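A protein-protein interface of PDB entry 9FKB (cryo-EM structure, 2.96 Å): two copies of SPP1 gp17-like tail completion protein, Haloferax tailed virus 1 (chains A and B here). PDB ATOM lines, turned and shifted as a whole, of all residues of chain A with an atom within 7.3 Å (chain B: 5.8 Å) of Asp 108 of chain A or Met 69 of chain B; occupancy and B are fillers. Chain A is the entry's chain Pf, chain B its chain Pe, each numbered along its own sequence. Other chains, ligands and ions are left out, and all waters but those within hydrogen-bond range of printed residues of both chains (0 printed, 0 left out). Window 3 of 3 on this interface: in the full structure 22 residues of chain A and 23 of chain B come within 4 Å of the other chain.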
ATOM      1  N   SER A 104     -16.308   0.415   5.826  1.00  0.00           N
ATOM      2  CA  SER A 104     -15.729  -0.839   6.293  1.00  0.00           C
ATOM      3  C   SER A 104     -14.566  -0.605   7.270  1.00  0.00           C
ATOM      4  O   SER A 104     -13.964  -1.563   7.753  1.00  0.00           O
ATOM      5  CB  SER A 104     -15.329  -1.734   5.147  1.00  0.00           C
ATOM      6  OG  SER A 104     -14.149  -1.256   4.508  1.00  0.00           O
ATOM      7  N   GLU A 105     -14.199   0.645   7.543  1.00  0.00           N
ATOM      8  CA  GLU A 105     -13.604   0.941   8.839  1.00  0.00           C
ATOM      9  C   GLU A 105     -14.732   0.849   9.873  1.00  0.00           C
ATOM     10  O   GLU A 105     -15.854   0.525   9.521  1.00  0.00           O
ATOM     11  CB  GLU A 105     -12.971   2.332   8.842  1.00  0.00           C
ATOM     12  CG  GLU A 105     -11.830   2.499   7.856  1.00  0.00           C
ATOM     13  CD  GLU A 105     -11.029   3.787   8.033  1.00  0.00           C
ATOM     14  OE1 GLU A 105     -11.123   4.401   9.127  1.00  0.00           O
ATOM     15  OE2 GLU A 105     -10.298   4.187   7.079  1.00  0.00           O
ATOM     16  N   TYR A 106     -14.477   1.135  11.152  1.00  0.00           N
ATOM     17  CA  TYR A 106     -15.552   1.209  12.154  1.00  0.00           C
ATOM     18  C   TYR A 106     -16.258  -0.126  12.454  1.00  0.00           C
ATOM     19  O   TYR A 106     -17.043  -0.175  13.411  1.00  0.00           O
ATOM     20  CB  TYR A 106     -16.593   2.286  11.796  1.00  0.00           C
ATOM     21  CG  TYR A 106     -15.987   3.572  11.284  1.00  0.00           C
ATOM     22  CD1 TYR A 106     -15.160   4.373  12.086  1.00  0.00           C
ATOM     23  CD2 TYR A 106     -16.184   3.941   9.964  1.00  0.00           C
ATOM     24  CE1 TYR A 106     -14.567   5.521  11.574  1.00  0.00           C
ATOM     25  CE2 TYR A 106     -15.607   5.100   9.451  1.00  0.00           C
ATOM     26  CZ  TYR A 106     -14.798   5.894  10.256  1.00  0.00           C
ATOM     27  OH  TYR A 106     -14.232   7.042   9.765  1.00  0.00           O
ATOM     28  N   LEU A 107     -15.962  -1.200  11.698  1.00  0.00           N
ATOM     29  CA  LEU A 107     -16.791  -2.399  11.598  1.00  0.00           C
ATOM     30  C   LEU A 107     -17.134  -3.007  12.952  1.00  0.00           C
ATOM     31  O   LEU A 107     -18.226  -3.557  13.111  1.00  0.00           O
ATOM     32  CB  LEU A 107     -16.087  -3.444  10.736  1.00  0.00           C
ATOM     33  CG  LEU A 107     -16.462  -3.458   9.258  1.00  0.00           C
ATOM     34  CD1 LEU A 107     -15.524  -4.380   8.498  1.00  0.00           C
ATOM     35  CD2 LEU A 107     -17.889  -3.950   9.044  1.00  0.00           C
ATOM     36  N   ASP A 108     -16.187  -2.947  13.903  1.00  0.00           N
ATOM     37  CA  ASP A 108     -16.420  -3.466  15.244  1.00  0.00           C
ATOM     38  C   ASP A 108     -15.846  -2.521  16.298  1.00  0.00           C
ATOM     39  O   ASP A 108     -15.189  -2.958  17.242  1.00  0.00           O
ATOM     40  CB  ASP A 108     -15.897  -4.904  15.383  1.00  0.00           C
ATOM     41  CG  ASP A 108     -16.532  -5.904  14.433  1.00  0.00           C
ATOM     42  OD1 ASP A 108     -17.754  -6.127  14.547  1.00  0.00           O
ATOM     43  OD2 ASP A 108     -15.784  -6.456  13.595  1.00  0.00           O
ATOM     44  N   ASP A 109     -16.107  -1.219  16.152  1.00  0.00           N
ATOM     45  CA  ASP A 109     -15.886  -0.271  17.238  1.00  0.00           C
ATOM     46  C   ASP A 109     -16.626  -0.733  18.499  1.00  0.00           C
ATOM     47  O   ASP A 109     -17.832  -0.854  18.498  1.00  0.00           O
ATOM     48  CB  ASP A 109     -16.533   1.077  16.895  1.00  0.00           C
ATOM     49  CG  ASP A 109     -15.687   2.068  16.122  1.00  0.00           C
ATOM     50  OD1 ASP A 109     -14.577   1.694  15.669  1.00  0.00           O
ATOM     51  OD2 ASP A 109     -16.133   3.237  16.051  1.00  0.00           O
ATOM     52  N   ASN A 110     -15.962  -0.970  19.617  1.00  0.00           N
ATOM     53  CA  ASN A 110     -16.651  -0.961  20.901  1.00  0.00           C
ATOM     54  C   ASN A 110     -16.916   0.506  21.294  1.00  0.00           C
ATOM     55  O   ASN A 110     -16.408   1.003  22.307  1.00  0.00           O
ATOM     56  CB  ASN A 110     -15.837  -1.763  21.933  1.00  0.00           C
ATOM     57  CG  ASN A 110     -14.361  -1.384  21.954  1.00  0.00           C
ATOM     58  OD1 ASN A 110     -13.562  -1.884  21.159  1.00  0.00           O
ATOM     59  ND2 ASN A 110     -13.972  -0.493  22.859  1.00  0.00           N
ATOM     60  N   GLU A 111     -17.650   1.243  20.453  1.00  0.00           N
ATOM     61  CA  GLU A 111     -17.937   2.672  20.585  1.00  0.00           C
ATOM     62  C   GLU A 111     -16.673   3.551  20.637  1.00  0.00           C
ATOM     63  O   GLU A 111     -16.619   4.557  21.355  1.00  0.00           O
ATOM     64  CB  GLU A 111     -18.889   2.951  21.753  1.00  0.00           C
ATOM     65  CG  GLU A 111     -20.203   2.176  21.683  1.00  0.00           C
ATOM     66  CD  GLU A 111     -21.257   2.570  22.712  1.00  0.00           C
ATOM     67  OE1 GLU A 111     -21.246   3.741  23.167  1.00  0.00           O
ATOM     68  OE2 GLU A 111     -22.116   1.709  23.045  1.00  0.00           O
ATOM     69  N   VAL A 112     -15.648   3.190  19.854  1.00  0.00           N
ATOM     70  CA  VAL A 112     -14.371   3.902  19.829  1.00  0.00           C
ATOM     71  C   VAL A 112     -14.494   5.221  19.055  1.00  0.00           C
ATOM     72  O   VAL A 112     -14.356   6.298  19.634  1.00  0.00           O
ATOM     73  CB  VAL A 112     -13.224   3.018  19.287  1.00  0.00           C
ATOM     74  CG1 VAL A 112     -11.890   3.758  19.311  1.00  0.00           C
ATOM     75  CG2 VAL A 112     -13.098   1.700  20.054  1.00  0.00           C
ATOM     76  N   THR A 114     -17.260   5.800  16.618  1.00  0.00           N
ATOM     77  CA  THR A 114     -18.705   5.950  16.536  1.00  0.00           C
ATOM     78  C   THR A 114     -19.380   5.734  17.890  1.00  0.00           C
ATOM     79  O   THR A 114     -18.798   5.161  18.805  1.00  0.00           O
ATOM     80  CB  THR A 114     -19.285   4.900  15.579  1.00  0.00           C
ATOM     81  OG1 THR A 114     -18.884   3.585  15.966  1.00  0.00           O
ATOM     82  CG2 THR A 114     -18.840   5.084  14.151  1.00  0.00           C
ATOM     83  N   TYR A 116     -21.498   3.413  18.371  1.00  0.00           N
ATOM     84  CA  TYR A 116     -22.076   2.117  18.027  1.00  0.00           C
ATOM     85  C   TYR A 116     -21.084   0.972  18.232  1.00  0.00           C
ATOM     86  O   TYR A 116     -19.880   1.181  18.273  1.00  0.00           O
ATOM     87  CB  TYR A 116     -22.519   2.152  16.567  1.00  0.00           C
ATOM     88  CG  TYR A 116     -23.750   2.979  16.331  1.00  0.00           C
ATOM     89  CD1 TYR A 116     -24.957   2.539  16.842  1.00  0.00           C
ATOM     90  CD2 TYR A 116     -23.734   4.163  15.599  1.00  0.00           C
ATOM     91  CE1 TYR A 116     -26.129   3.255  16.632  1.00  0.00           C
ATOM     92  CE2 TYR A 116     -24.899   4.894  15.386  1.00  0.00           C
ATOM     93  CZ  TYR A 116     -26.105   4.442  15.914  1.00  0.00           C
ATOM     94  OH  TYR A 116     -27.299   5.095  15.731  1.00  0.00           O
ATOM     95  N   SER A 117     -21.609  -0.254  18.367  1.00  0.00           N
ATOM     96  CA  SER A 117     -20.810  -1.476  18.412  1.00  0.00           C
ATOM     97  C   SER A 117     -20.350  -1.900  17.016  1.00  0.00           C
ATOM     98  O   SER A 117     -19.351  -2.604  16.851  1.00  0.00           O
ATOM     99  CB  SER A 117     -21.603  -2.617  19.019  1.00  0.00           C
ATOM    100  OG  SER A 117     -22.109  -2.292  20.303  1.00  0.00           O
ATOM    101  N   ASP A 118     -21.134  -1.534  16.008  1.00  0.00           N
ATOM    102  CA  ASP A 118     -21.011  -2.071  14.665  1.00  0.00           C
ATOM    103  C   ASP A 118     -21.661  -1.084  13.704  1.00  0.00           C
ATOM    104  O   ASP A 118     -22.811  -0.703  13.891  1.00  0.00           O
ATOM    105  CB  ASP A 118     -21.715  -3.432  14.607  1.00  0.00           C
ATOM    106  CG  ASP A 118     -21.924  -4.055  13.226  1.00  0.00           C
ATOM    107  OD1 ASP A 118     -21.575  -3.427  12.218  1.00  0.00           O
ATOM    108  OD2 ASP A 118     -22.489  -5.172  13.166  1.00  0.00           O
ATOM    109  N   VAL A 119     -20.890  -0.643  12.706  1.00  0.00           N
ATOM    110  CA  VAL A 119     -21.417  -0.039  11.497  1.00  0.00           C
ATOM    111  C   VAL A 119     -20.931  -0.891  10.328  1.00  0.00           C
ATOM    112  O   VAL A 119     -19.728  -1.048  10.166  1.00  0.00           O
ATOM    113  CB  VAL A 119     -20.922   1.412  11.364  1.00  0.00           C
ATOM    114  CG1 VAL A 119     -21.329   2.015  10.025  1.00  0.00           C
ATOM    115  CG2 VAL A 119     -21.424   2.286  12.506  1.00  0.00           C
ATOM    116  N   ARG B  66     -20.949 -10.900   6.789  1.00  0.00           N
ATOM    117  CA  ARG B  66     -19.729 -10.996   7.577  1.00  0.00           C
ATOM    118  C   ARG B  66     -19.130 -12.391   7.390  1.00  0.00           C
ATOM    119  O   ARG B  66     -19.855 -13.396   7.482  1.00  0.00           O
ATOM    120  CB  ARG B  66     -20.067 -10.762   9.055  1.00  0.00           C
ATOM    121  CG  ARG B  66     -20.418  -9.323   9.399  1.00  0.00           C
ATOM    122  CD  ARG B  66     -19.200  -8.403   9.281  1.00  0.00           C
ATOM    123  NE  ARG B  66     -18.043  -8.717  10.105  1.00  0.00           N
ATOM    124  CZ  ARG B  66     -17.692  -8.097  11.233  1.00  0.00           C
ATOM    125  NH1 ARG B  66     -16.603  -8.493  11.866  1.00  0.00           N
ATOM    126  NH2 ARG B  66     -18.379  -7.073  11.733  1.00  0.00           N
ATOM    127  N   PHE B  67     -17.804 -12.471   7.189  1.00  0.00           N
ATOM    128  CA  PHE B  67     -17.195 -13.786   7.017  1.00  0.00           C
ATOM    129  C   PHE B  67     -16.756 -14.416   8.345  1.00  0.00           C
ATOM    130  O   PHE B  67     -16.784 -15.637   8.523  1.00  0.00           O
ATOM    131  CB  PHE B  67     -16.004 -13.683   6.080  1.00  0.00           C
ATOM    132  CG  PHE B  67     -15.413 -15.014   5.690  1.00  0.00           C
ATOM    133  CD1 PHE B  67     -16.158 -15.946   4.961  1.00  0.00           C
ATOM    134  CD2 PHE B  67     -14.108 -15.319   6.064  1.00  0.00           C
ATOM    135  CE1 PHE B  67     -15.616 -17.179   4.627  1.00  0.00           C
ATOM    136  CE2 PHE B  67     -13.544 -16.536   5.686  1.00  0.00           C
ATOM    137  CZ  PHE B  67     -14.301 -17.453   4.967  1.00  0.00           C
ATOM    138  N   SER B  68     -16.303 -13.561   9.279  1.00  0.00           N
ATOM    139  CA  SER B  68     -15.689 -14.015  10.519  1.00  0.00           C
ATOM    140  C   SER B  68     -15.638 -12.874  11.527  1.00  0.00           C
ATOM    141  O   SER B  68     -15.956 -11.741  11.175  1.00  0.00           O
ATOM    142  CB  SER B  68     -14.280 -14.508  10.254  1.00  0.00           C
ATOM    143  OG  SER B  68     -13.386 -13.448   9.943  1.00  0.00           O
ATOM    144  N   MET B  69     -15.176 -13.158  12.756  1.00  0.00           N
ATOM    145  CA  MET B  69     -15.013 -12.110  13.751  1.00  0.00           C
ATOM    146  C   MET B  69     -13.960 -11.093  13.327  1.00  0.00           C
ATOM    147  O   MET B  69     -13.999  -9.955  13.807  1.00  0.00           O
ATOM    148  CB  MET B  69     -14.615 -12.686  15.109  1.00  0.00           C
ATOM    149  CG  MET B  69     -15.735 -13.509  15.712  1.00  0.00           C
ATOM    150  SD  MET B  69     -15.610 -13.740  17.494  1.00  0.00           S
ATOM    151  CE  MET B  69     -16.180 -15.438  17.593  1.00  0.00           C
ATOM    152  N   ASP B  70     -13.031 -11.468  12.436  1.00  0.00           N
ATOM    153  CA  ASP B  70     -11.888 -10.629  12.108  1.00  0.00           C
ATOM    154  C   ASP B  70     -12.286  -9.362  11.340  1.00  0.00           C
ATOM    155  O   ASP B  70     -11.604  -8.329  11.448  1.00  0.00           O
ATOM    156  CB  ASP B  70     -10.830 -11.409  11.326  1.00  0.00           C
ATOM    157  CG  ASP B  70     -10.102 -12.519  12.079  1.00  0.00           C
ATOM    158  OD1 ASP B  70     -10.666 -13.118  13.040  1.00  0.00           O
ATOM    159  OD2 ASP B  70      -8.913 -12.784  11.717  1.00  0.00           O
ATOM    160  N   GLY B  71     -13.409  -9.408  10.608  1.00  0.00           N
ATOM    161  CA  GLY B  71     -13.891  -8.281   9.822  1.00  0.00           C
ATOM    162  C   GLY B  71     -13.002  -7.926   8.625  1.00  0.00           C
ATOM    163  O   GLY B  71     -13.267  -6.954   7.915  1.00  0.00           O
ATOM    164  N   LYS B 155     -10.970  -1.969   7.764  1.00  0.00           N
ATOM    165  CA  LYS B 155     -10.760  -2.073   9.211  1.00  0.00           C
ATOM    166  C   LYS B 155      -9.312  -2.426   9.584  1.00  0.00           C
ATOM    167  O   LYS B 155      -8.766  -1.874  10.547  1.00  0.00           O
ATOM    168  CB  LYS B 155     -11.741  -3.098   9.782  1.00  0.00           C
ATOM    169  CG  LYS B 155     -11.534  -3.469  11.240  1.00  0.00           C
ATOM    170  CD  LYS B 155     -12.483  -4.551  11.753  1.00  0.00           C
ATOM    171  CE  LYS B 155     -12.064  -5.127  13.093  1.00  0.00           C
ATOM    172  NZ  LYS B 155     -10.902  -6.043  12.972  1.00  0.00           N
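Of the printed residues of chain B, Asp 108 of chain A touches Arg 66, Met 69 and Lys 155.
Of chain A, only Asp 108 comes within 4 Å of Met 69 of chain B.
Printed residues of chain A within 4 Å of Lys 155 of chain B: Ser 104, Leu 107 and Asp 108.
Printed residues of chain B within 4 Å of Leu 107 of chain A: Arg 66, Gly 71 and Lys 155.
Of the printed residues of chain A, Arg 66 of chain B touches Leu 107 (3.8 Å) and Asp 108 (2.8 Å).
Of the printed residues of chain B, Ser 104 of chain A touches Lys 155.
The nearest printed residue of chain A that does not touch Gly 71 of chain B is Asp 108 of chain A (4.6 Å).
Arg 66 of chain B touches Leu 107 of chain A.
CD1 of Leu 107 of chain A touches O of Gly 71 of chain B (3.5 Å).
Leu 107 of chain A touches Lys 155 of chain B.
Met 69 of chain B touches Asp 108 of chain A.
Lys 155 of chain B touches Asp 108 of chain A (CE to OD2, 3.98 Å).
The backbone carbonyl oxygen of Asp 70 of chain B is in hydrogen-bond range of the side-chain amino group of Lys 155 of chain B (2.8 Å).
The backbone carbonyl oxygen of Ser 68 of chain B lies within hydrogen-bond range of the guanidinium group of Arg 66 of chain B.
NH1 of Arg 66 of chain B lies within salt-bridge range of OD2 of Asp 108 of chain A (2.8 Å).
O of Ser 104 of chain A is in hydrogen-bond range of N of Lys 155 of chain B.
Of the 14 printed residues of chain A, 3 touch a printed residue of chain B.
Printed residues of chain A that touch a printed residue of chain B: Ser 104, Leu 107 and Asp 108.
Along chain A the printed residues that touch a printed residue of chain B span positions 104 to 108.
Among the printed residues, Asp or Glu carboxylates within 4 Å of a Lys or Arg side-chain nitrogen of the other chain: Asp 108 of chain A with Arg 66 of chain B (2.8 Å).
No position is printed for both chains.
Of the 7 pairs that touch across the chains among the printed residues, none has its exchanged pair printed and touching as well.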
